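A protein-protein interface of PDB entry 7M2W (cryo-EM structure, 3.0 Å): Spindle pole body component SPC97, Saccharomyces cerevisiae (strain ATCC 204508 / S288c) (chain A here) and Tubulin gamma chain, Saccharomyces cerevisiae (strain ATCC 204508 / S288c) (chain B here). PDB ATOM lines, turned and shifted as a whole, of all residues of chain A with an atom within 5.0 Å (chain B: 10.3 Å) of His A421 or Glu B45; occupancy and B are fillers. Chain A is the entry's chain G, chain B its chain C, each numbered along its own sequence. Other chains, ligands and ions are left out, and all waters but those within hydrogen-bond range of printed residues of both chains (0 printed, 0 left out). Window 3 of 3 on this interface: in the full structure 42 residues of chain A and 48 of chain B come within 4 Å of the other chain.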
ATOM      1  N   ASN A 417      -2.993  14.781  29.784  1.00  0.00           N
ATOM      2  CA  ASN A 417      -3.726  15.554  28.789  1.00  0.00           C
ATOM      3  C   ASN A 417      -5.229  15.333  28.913  1.00  0.00           C
ATOM      4  O   ASN A 417      -6.019  16.261  28.705  1.00  0.00           O
ATOM      5  CB  ASN A 417      -3.235  15.195  27.389  1.00  0.00           C
ATOM      6  CG  ASN A 417      -3.945  15.973  26.305  1.00  0.00           C
ATOM      7  OD1 ASN A 417      -4.871  15.468  25.672  1.00  0.00           O
ATOM      8  ND2 ASN A 417      -3.517  17.209  26.084  1.00  0.00           N
ATOM      9  N   VAL A 418      -5.647  14.115  29.261  1.00  0.00           N
ATOM     10  CA  VAL A 418      -7.070  13.855  29.448  1.00  0.00           C
ATOM     11  C   VAL A 418      -7.605  14.650  30.629  1.00  0.00           C
ATOM     12  O   VAL A 418      -8.696  15.228  30.567  1.00  0.00           O
ATOM     13  CB  VAL A 418      -7.324  12.349  29.623  1.00  0.00           C
ATOM     14  CG1 VAL A 418      -8.806  12.052  29.511  1.00  0.00           C
ATOM     15  CG2 VAL A 418      -6.544  11.558  28.593  1.00  0.00           C
ATOM     16  N   LEU A 419      -6.843  14.705  31.721  1.00  0.00           N
ATOM     17  CA  LEU A 419      -7.264  15.498  32.869  1.00  0.00           C
ATOM     18  C   LEU A 419      -7.239  16.983  32.544  1.00  0.00           C
ATOM     19  O   LEU A 419      -8.099  17.740  33.006  1.00  0.00           O
ATOM     20  CB  LEU A 419      -6.375  15.192  34.071  1.00  0.00           C
ATOM     21  CG  LEU A 419      -6.565  13.780  34.617  1.00  0.00           C
ATOM     22  CD1 LEU A 419      -5.464  13.428  35.595  1.00  0.00           C
ATOM     23  CD2 LEU A 419      -7.928  13.657  35.258  1.00  0.00           C
ATOM     24  N   LYS A 420      -6.267  17.416  31.739  1.00  0.00           N
ATOM     25  CA  LYS A 420      -6.223  18.808  31.307  1.00  0.00           C
ATOM     26  C   LYS A 420      -7.471  19.171  30.517  1.00  0.00           C
ATOM     27  O   LYS A 420      -8.078  20.222  30.741  1.00  0.00           O
ATOM     28  CB  LYS A 420      -4.961  19.051  30.479  1.00  0.00           C
ATOM     29  CG  LYS A 420      -4.884  20.414  29.819  1.00  0.00           C
ATOM     30  CD  LYS A 420      -3.655  20.506  28.926  1.00  0.00           C
ATOM     31  CE  LYS A 420      -3.624  21.809  28.148  1.00  0.00           C
ATOM     32  NZ  LYS A 420      -2.559  21.807  27.106  1.00  0.00           N
ATOM     33  N   HIS A 421      -7.889  18.294  29.604  1.00  0.00           N
ATOM     34  CA  HIS A 421      -9.077  18.579  28.806  1.00  0.00           C
ATOM     35  C   HIS A 421     -10.344  18.503  29.648  1.00  0.00           C
ATOM     36  O   HIS A 421     -11.287  19.271  29.433  1.00  0.00           O
ATOM     37  CB  HIS A 421      -9.155  17.618  27.622  1.00  0.00           C
ATOM     38  CG  HIS A 421      -8.078  17.828  26.606  1.00  0.00           C
ATOM     39  ND1 HIS A 421      -7.957  17.048  25.477  1.00  0.00           N
ATOM     40  CD2 HIS A 421      -7.077  18.737  26.543  1.00  0.00           C
ATOM     41  CE1 HIS A 421      -6.927  17.465  24.765  1.00  0.00           C
ATOM     42  NE2 HIS A 421      -6.374  18.488  25.391  1.00  0.00           N
ATOM     43  N   LEU A 422     -10.377  17.608  30.637  1.00  0.00           N
ATOM     44  CA  LEU A 422     -11.541  17.538  31.513  1.00  0.00           C
ATOM     45  C   LEU A 422     -11.641  18.778  32.389  1.00  0.00           C
ATOM     46  O   LEU A 422     -12.744  19.246  32.692  1.00  0.00           O
ATOM     47  CB  LEU A 422     -11.477  16.279  32.370  1.00  0.00           C
ATOM     48  CG  LEU A 422     -11.991  15.017  31.686  1.00  0.00           C
ATOM     49  CD1 LEU A 422     -11.839  13.831  32.603  1.00  0.00           C
ATOM     50  CD2 LEU A 422     -13.437  15.197  31.278  1.00  0.00           C
ATOM     51  N   GLN A 423     -10.499  19.326  32.798  1.00  0.00           N
ATOM     52  CA  GLN A 423     -10.508  20.560  33.572  1.00  0.00           C
ATOM     53  C   GLN A 423     -10.829  21.756  32.687  1.00  0.00           C
ATOM     54  O   GLN A 423     -11.395  22.749  33.156  1.00  0.00           O
ATOM     55  CB  GLN A 423      -9.162  20.741  34.268  1.00  0.00           C
ATOM     56  CG  GLN A 423      -8.935  19.768  35.405  1.00  0.00           C
ATOM     57  CD  GLN A 423      -7.471  19.550  35.701  1.00  0.00           C
ATOM     58  OE1 GLN A 423      -6.619  19.713  34.830  1.00  0.00           O
ATOM     59  NE2 GLN A 423      -7.168  19.184  36.936  1.00  0.00           N
ATOM     60  N   GLN A 424     -10.476  21.678  31.404  1.00  0.00           N
ATOM     61  CA  GLN A 424     -10.877  22.723  30.470  1.00  0.00           C
ATOM     62  C   GLN A 424     -12.375  22.693  30.221  1.00  0.00           C
ATOM     63  O   GLN A 424     -12.989  23.742  30.006  1.00  0.00           O
ATOM     64  CB  GLN A 424     -10.130  22.572  29.147  1.00  0.00           C
ATOM     65  CG  GLN A 424      -8.675  22.974  29.191  1.00  0.00           C
ATOM     66  CD  GLN A 424      -7.985  22.770  27.860  1.00  0.00           C
ATOM     67  OE1 GLN A 424      -8.619  22.417  26.868  1.00  0.00           O
ATOM     68  NE2 GLN A 424      -6.678  22.991  27.833  1.00  0.00           N
ATOM     69  N   ILE A 425     -12.980  21.508  30.242  1.00  0.00           N
ATOM     70  CA  ILE A 425     -14.412  21.411  29.978  1.00  0.00           C
ATOM     71  C   ILE A 425     -15.219  21.780  31.214  1.00  0.00           C
ATOM     72  O   ILE A 425     -16.136  22.604  31.146  1.00  0.00           O
ATOM     73  CB  ILE A 425     -14.780  20.003  29.483  1.00  0.00           C
ATOM     74  CG1 ILE A 425     -14.109  19.698  28.147  1.00  0.00           C
ATOM     75  CG2 ILE A 425     -16.282  19.877  29.348  1.00  0.00           C
ATOM     76  CD1 ILE A 425     -14.484  18.345  27.596  1.00  0.00           C
ATOM     77  N   ASN A 473     -11.223  20.700  18.041  1.00  0.00           N
ATOM     78  CA  ASN A 473     -10.037  19.922  17.718  1.00  0.00           C
ATOM     79  C   ASN A 473     -10.392  18.441  17.677  1.00  0.00           C
ATOM     80  O   ASN A 473     -11.071  17.951  18.592  1.00  0.00           O
ATOM     81  CB  ASN A 473      -8.934  20.181  18.743  1.00  0.00           C
ATOM     82  CG  ASN A 473      -7.603  19.558  18.349  1.00  0.00           C
ATOM     83  OD1 ASN A 473      -7.502  18.349  18.143  1.00  0.00           O
ATOM     84  ND2 ASN A 473      -6.573  20.388  18.244  1.00  0.00           N
ATOM     85  N   ASN A 475      -8.296  15.801  17.944  1.00  0.00           N
ATOM     86  CA  ASN A 475      -7.505  15.048  18.909  1.00  0.00           C
ATOM     87  C   ASN A 475      -7.964  15.251  20.345  1.00  0.00           C
ATOM     88  O   ASN A 475      -7.382  14.650  21.254  1.00  0.00           O
ATOM     89  CB  ASN A 475      -6.028  15.426  18.789  1.00  0.00           C
ATOM     90  CG  ASN A 475      -5.383  14.854  17.546  1.00  0.00           C
ATOM     91  OD1 ASN A 475      -5.969  14.020  16.860  1.00  0.00           O
ATOM     92  ND2 ASN A 475      -4.168  15.298  17.253  1.00  0.00           N
ATOM     93  N   ASN A 476      -8.978  16.084  20.574  1.00  0.00           N
ATOM     94  CA  ASN A 476      -9.524  16.296  21.912  1.00  0.00           C
ATOM     95  C   ASN A 476     -10.701  15.343  22.082  1.00  0.00           C
ATOM     96  O   ASN A 476     -11.856  15.667  21.803  1.00  0.00           O
ATOM     97  CB  ASN A 476      -9.929  17.753  22.101  1.00  0.00           C
ATOM     98  CG  ASN A 476     -10.497  18.033  23.474  1.00  0.00           C
ATOM     99  OD1 ASN A 476     -11.521  17.478  23.866  1.00  0.00           O
ATOM    100  ND2 ASN A 476      -9.837  18.915  24.213  1.00  0.00           N
ATOM    101  N   LEU A 477     -10.387  14.133  22.551  1.00  0.00           N
ATOM    102  CA  LEU A 477     -11.401  13.090  22.658  1.00  0.00           C
ATOM    103  C   LEU A 477     -12.525  13.491  23.607  1.00  0.00           C
ATOM    104  O   LEU A 477     -13.667  13.046  23.451  1.00  0.00           O
ATOM    105  CB  LEU A 477     -10.756  11.782  23.116  1.00  0.00           C
ATOM    106  CG  LEU A 477     -11.689  10.585  23.287  1.00  0.00           C
ATOM    107  CD1 LEU A 477     -12.515  10.366  22.031  1.00  0.00           C
ATOM    108  CD2 LEU A 477     -10.895   9.342  23.631  1.00  0.00           C
ATOM    109  N   MET A 478     -12.224  14.336  24.593  1.00  0.00           N
ATOM    110  CA  MET A 478     -13.233  14.673  25.589  1.00  0.00           C
ATOM    111  C   MET A 478     -14.296  15.605  25.028  1.00  0.00           C
ATOM    112  O   MET A 478     -15.487  15.406  25.284  1.00  0.00           O
ATOM    113  CB  MET A 478     -12.571  15.288  26.819  1.00  0.00           C
ATOM    114  CG  MET A 478     -11.697  14.312  27.584  1.00  0.00           C
ATOM    115  SD  MET A 478     -12.661  13.052  28.438  1.00  0.00           S
ATOM    116  CE  MET A 478     -12.006  11.563  27.695  1.00  0.00           C
ATOM    117  N   SER B  37       4.569  30.416  12.223  1.00  0.00           N
ATOM    118  CA  SER B  37       4.716  29.869  13.565  1.00  0.00           C
ATOM    119  C   SER B  37       6.063  29.182  13.735  1.00  0.00           C
ATOM    120  O   SER B  37       6.402  28.253  12.998  1.00  0.00           O
ATOM    121  CB  SER B  37       3.585  28.883  13.857  1.00  0.00           C
ATOM    122  OG  SER B  37       3.732  28.309  15.142  1.00  0.00           O
ATOM    123  N   LEU B  39       6.747  27.200  15.910  1.00  0.00           N
ATOM    124  CA  LEU B  39       6.392  25.964  16.584  1.00  0.00           C
ATOM    125  C   LEU B  39       6.346  24.808  15.594  1.00  0.00           C
ATOM    126  O   LEU B  39       5.833  24.954  14.481  1.00  0.00           O
ATOM    127  CB  LEU B  39       5.026  26.089  17.264  1.00  0.00           C
ATOM    128  CG  LEU B  39       4.870  27.135  18.367  1.00  0.00           C
ATOM    129  CD1 LEU B  39       3.426  27.204  18.833  1.00  0.00           C
ATOM    130  CD2 LEU B  39       5.795  26.825  19.527  1.00  0.00           C
ATOM    131  N   PRO B  40       6.884  23.649  15.970  1.00  0.00           N
ATOM    132  CA  PRO B  40       6.750  22.467  15.112  1.00  0.00           C
ATOM    133  C   PRO B  40       5.292  22.056  14.978  1.00  0.00           C
ATOM    134  O   PRO B  40       4.549  21.976  15.959  1.00  0.00           O
ATOM    135  CB  PRO B  40       7.571  21.398  15.844  1.00  0.00           C
ATOM    136  CG  PRO B  40       8.494  22.167  16.736  1.00  0.00           C
ATOM    137  CD  PRO B  40       7.729  23.384  17.147  1.00  0.00           C
ATOM    138  N   ASP B  41       4.889  21.787  13.736  1.00  0.00           N
ATOM    139  CA  ASP B  41       3.511  21.447  13.406  1.00  0.00           C
ATOM    140  C   ASP B  41       3.098  20.070  13.919  1.00  0.00           C
ATOM    141  O   ASP B  41       1.961  19.647  13.687  1.00  0.00           O
ATOM    142  CB  ASP B  41       3.296  21.540  11.894  1.00  0.00           C
ATOM    143  CG  ASP B  41       4.221  20.625  11.110  1.00  0.00           C
ATOM    144  OD1 ASP B  41       5.090  19.970  11.725  1.00  0.00           O
ATOM    145  OD2 ASP B  41       4.079  20.560   9.870  1.00  0.00           O
ATOM    146  N   SER B  42       4.001  19.364  14.605  1.00  0.00           N
ATOM    147  CA  SER B  42       3.717  18.027  15.118  1.00  0.00           C
ATOM    148  C   SER B  42       2.513  17.983  16.052  1.00  0.00           C
ATOM    149  O   SER B  42       1.948  16.901  16.246  1.00  0.00           O
ATOM    150  CB  SER B  42       4.945  17.478  15.846  1.00  0.00           C
ATOM    151  OG  SER B  42       5.438  18.412  16.791  1.00  0.00           O
ATOM    152  N   SER B  43       2.110  19.112  16.633  1.00  0.00           N
ATOM    153  CA  SER B  43       0.980  19.151  17.548  1.00  0.00           C
ATOM    154  C   SER B  43      -0.118  20.028  16.967  1.00  0.00           C
ATOM    155  O   SER B  43       0.163  21.024  16.295  1.00  0.00           O
ATOM    156  CB  SER B  43       1.394  19.680  18.928  1.00  0.00           C
ATOM    157  OG  SER B  43       0.272  20.141  19.660  1.00  0.00           O
ATOM    158  N   THR B  44      -1.366  19.649  17.229  1.00  0.00           N
ATOM    159  CA  THR B  44      -2.527  20.416  16.800  1.00  0.00           C
ATOM    160  C   THR B  44      -3.273  21.055  17.964  1.00  0.00           C
ATOM    161  O   THR B  44      -4.422  21.473  17.791  1.00  0.00           O
ATOM    162  CB  THR B  44      -3.488  19.528  16.001  1.00  0.00           C
ATOM    163  OG1 THR B  44      -4.013  18.500  16.849  1.00  0.00           O
ATOM    164  CG2 THR B  44      -2.769  18.889  14.823  1.00  0.00           C
ATOM    165  N   GLU B  45      -2.654  21.140  19.137  1.00  0.00           N
ATOM    166  CA  GLU B  45      -3.278  21.715  20.319  1.00  0.00           C
ATOM    167  C   GLU B  45      -2.493  22.942  20.761  1.00  0.00           C
ATOM    168  O   GLU B  45      -1.289  22.851  21.024  1.00  0.00           O
ATOM    169  CB  GLU B  45      -3.337  20.691  21.452  1.00  0.00           C
ATOM    170  CG  GLU B  45      -4.045  21.162  22.719  1.00  0.00           C
ATOM    171  CD  GLU B  45      -5.397  21.799  22.448  1.00  0.00           C
ATOM    172  OE1 GLU B  45      -5.444  23.004  22.124  1.00  0.00           O
ATOM    173  OE2 GLU B  45      -6.419  21.088  22.561  1.00  0.00           O
ATOM    174  N   ARG B  46      -3.173  24.084  20.842  1.00  0.00           N
ATOM    175  CA  ARG B  46      -2.564  25.327  21.284  1.00  0.00           C
ATOM    176  C   ARG B  46      -3.158  25.747  22.621  1.00  0.00           C
ATOM    177  O   ARG B  46      -4.317  25.455  22.925  1.00  0.00           O
ATOM    178  CB  ARG B  46      -2.758  26.448  20.255  1.00  0.00           C
ATOM    179  CG  ARG B  46      -1.995  26.245  18.957  1.00  0.00           C
ATOM    180  CD  ARG B  46      -0.510  26.524  19.135  1.00  0.00           C
ATOM    181  NE  ARG B  46      -0.226  27.938  19.366  1.00  0.00           N
ATOM    182  CZ  ARG B  46      -0.226  28.870  18.418  1.00  0.00           C
ATOM    183  NH1 ARG B  46      -0.494  28.544  17.162  1.00  0.00           N
ATOM    184  NH2 ARG B  46       0.046  30.130  18.727  1.00  0.00           N
ATOM    185  N   ASP B  47      -2.347  26.444  23.415  1.00  0.00           N
ATOM    186  CA  ASP B  47      -2.733  26.884  24.748  1.00  0.00           C
ATOM    187  C   ASP B  47      -3.300  28.298  24.756  1.00  0.00           C
ATOM    188  O   ASP B  47      -3.780  28.761  25.795  1.00  0.00           O
ATOM    189  CB  ASP B  47      -1.536  26.793  25.696  1.00  0.00           C
ATOM    190  CG  ASP B  47      -1.467  25.468  26.426  1.00  0.00           C
ATOM    191  OD1 ASP B  47      -2.519  24.994  26.902  1.00  0.00           O
ATOM    192  OD2 ASP B  47      -0.359  24.899  26.524  1.00  0.00           O
ATOM    193  N   ASP B  48      -3.262  28.991  23.620  1.00  0.00           N
ATOM    194  CA  ASP B  48      -3.619  30.400  23.563  1.00  0.00           C
ATOM    195  C   ASP B  48      -4.700  30.613  22.513  1.00  0.00           C
ATOM    196  O   ASP B  48      -5.073  29.697  21.773  1.00  0.00           O
ATOM    197  CB  ASP B  48      -2.390  31.262  23.261  1.00  0.00           C
ATOM    198  CG  ASP B  48      -1.765  30.930  21.924  1.00  0.00           C
ATOM    199  OD1 ASP B  48      -2.076  29.859  21.366  1.00  0.00           O
ATOM    200  OD2 ASP B  48      -0.955  31.740  21.430  1.00  0.00           O
ATOM    201  N   ASP B  49      -5.202  31.846  22.453  1.00  0.00           N
ATOM    202  CA  ASP B  49      -6.192  32.252  21.456  1.00  0.00           C
ATOM    203  C   ASP B  49      -5.615  33.445  20.703  1.00  0.00           C
ATOM    204  O   ASP B  49      -5.818  34.595  21.100  1.00  0.00           O
ATOM    205  CB  ASP B  49      -7.526  32.598  22.104  1.00  0.00           C
ATOM    206  CG  ASP B  49      -8.696  32.423  21.157  1.00  0.00           C
ATOM    207  OD1 ASP B  49      -8.534  31.728  20.134  1.00  0.00           O
ATOM    208  OD2 ASP B  49      -9.779  32.983  21.435  1.00  0.00           O
ATOM    209  N   PRO B 245      -5.942  32.718  27.801  1.00  0.00           N
ATOM    210  CA  PRO B 245      -7.130  32.854  28.645  1.00  0.00           C
ATOM    211  C   PRO B 245      -6.980  32.113  29.962  1.00  0.00           C
ATOM    212  O   PRO B 245      -6.156  31.209  30.106  1.00  0.00           O
ATOM    213  CB  PRO B 245      -8.248  32.249  27.788  1.00  0.00           C
ATOM    214  CG  PRO B 245      -7.659  32.119  26.400  1.00  0.00           C
ATOM    215  CD  PRO B 245      -6.209  31.880  26.625  1.00  0.00           C
ATOM    216  N   ARG B 358      -1.800  34.388  33.118  1.00  0.00           N
ATOM    217  CA  ARG B 358      -0.813  33.390  32.747  1.00  0.00           C
ATOM    218  C   ARG B 358       0.334  34.049  32.003  1.00  0.00           C
ATOM    219  O   ARG B 358       0.148  35.034  31.286  1.00  0.00           O
ATOM    220  CB  ARG B 358      -1.408  32.299  31.857  1.00  0.00           C
ATOM    221  CG  ARG B 358      -2.447  31.430  32.516  1.00  0.00           C
ATOM    222  CD  ARG B 358      -2.510  30.092  31.813  1.00  0.00           C
ATOM    223  NE  ARG B 358      -3.330  30.157  30.609  1.00  0.00           N
ATOM    224  CZ  ARG B 358      -2.926  29.740  29.415  1.00  0.00           C
ATOM    225  NH1 ARG B 358      -1.712  29.230  29.264  1.00  0.00           N
ATOM    226  NH2 ARG B 358      -3.734  29.834  28.370  1.00  0.00           N
ATOM    227  N   PRO B 361       3.177  30.560  27.457  1.00  0.00           N
ATOM    228  CA  PRO B 361       3.889  29.274  27.494  1.00  0.00           C
ATOM    229  C   PRO B 361       5.013  29.170  26.481  1.00  0.00           C
ATOM    230  O   PRO B 361       5.973  28.429  26.724  1.00  0.00           O
ATOM    231  CB  PRO B 361       2.785  28.251  27.201  1.00  0.00           C
ATOM    232  CG  PRO B 361       1.729  29.027  26.490  1.00  0.00           C
ATOM    233  CD  PRO B 361       1.765  30.400  27.077  1.00  0.00           C
ATOM    234  N   TYR B 362       4.928  29.884  25.359  1.00  0.00           N
ATOM    235  CA  TYR B 362       5.966  29.865  24.340  1.00  0.00           C
ATOM    236  C   TYR B 362       7.051  30.900  24.597  1.00  0.00           C
ATOM    237  O   TYR B 362       8.063  30.912  23.891  1.00  0.00           O
ATOM    238  CB  TYR B 362       5.347  30.078  22.957  1.00  0.00           C
ATOM    239  CG  TYR B 362       4.059  29.317  22.755  1.00  0.00           C
ATOM    240  CD1 TYR B 362       2.872  29.981  22.488  1.00  0.00           C
ATOM    241  CD2 TYR B 362       4.028  27.935  22.844  1.00  0.00           C
ATOM    242  CE1 TYR B 362       1.692  29.289  22.305  1.00  0.00           C
ATOM    243  CE2 TYR B 362       2.854  27.234  22.664  1.00  0.00           C
ATOM    244  CZ  TYR B 362       1.689  27.916  22.396  1.00  0.00           C
ATOM    245  OH  TYR B 362       0.518  27.217  22.218  1.00  0.00           O
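The side-chain amide oxygen (OD1) of Asn A473 is in hydrogen-bond range of the backbone NH (N) of Asn A475 (2.7 Å). The backbone NH (N) of Glu B45 is in hydrogen-bond range of the side-chain hydroxyl (OG) of Ser B43 (3.1 Å). The side-chain amide nitrogen of Asn A417 lies within hydrogen-bond range of a ring nitrogen (NE2) of His A421, at 3.2 Å. ND1 of His A421 sits at hydrogen-bond distance from ND2 of Asn A476 (2.9 Å). The guanidinium group of Arg B358 lies within hydrogen-bond range of the backbone carbonyl oxygen of Asp B47. The backbone NH of Asp B47 is in hydrogen-bond range of the side-chain hydroxyl of Tyr B362, at 3.2 Å.
Of chain B, only Asp B47 (3.2 Å) comes within 4 Å of Lys A420. His A421 touches just one residue of chain B: Glu B45 (3.8 Å). No residue of chain B comes within 4 Å of Gln A424. Printed residues of chain B within 4 Å of Asn A473: Thr B44. Printed residues of chain B within 4 Å of Asn A475: Thr B44 (3.2 Å). No residue of chain B comes within 4 Å of Asn A476. Of the printed residues of chain A, Thr B44 touches Asn A473 (2.5 Å) and Asn A475 (3.2 Å). Of the printed residues of chain A, Glu B45 touches His A421. Of the printed residues of chain A, Asp B47 touches Lys A420 (3.2 Å). The nearest residue of chain A that does not touch Glu B45 is Asn A473 (4.1 Å). The nearest printed residue of chain A that does not touch Thr B44 is Asn A476 (6.7 Å).
The backbone carbonyl oxygen of Thr B44 sits at hydrogen-bond distance from the side-chain amide nitrogen of Asn A473 (2.5 Å). The side-chain amino group (NZ) of Lys A420 is in salt-bridge range of the side-chain carboxylate (OD1) of Asp B47. OG1 of Thr B44 is in hydrogen-bond range of ND2 of Asn A475 (3.2 Å).
Of the 14 printed residues of chain A, 4 touch a printed residue of chain B. Hydrophobic or aromatic side chains of chain A within 4 Å of the printed part of chain B: His A421. Of the 16 printed residues of chain B, 3 touch a printed residue of chain A. Among the printed residues, 4 pairs touch across the chains. Among the printed residues, Asp or Glu carboxylates within 4 Å of a Lys or Arg side-chain nitrogen of the other chain: Lys A420 with Asp B47 (3.2 Å).
Glu B45 touches His A421 (OE2 to NE2, 3.8 Å).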
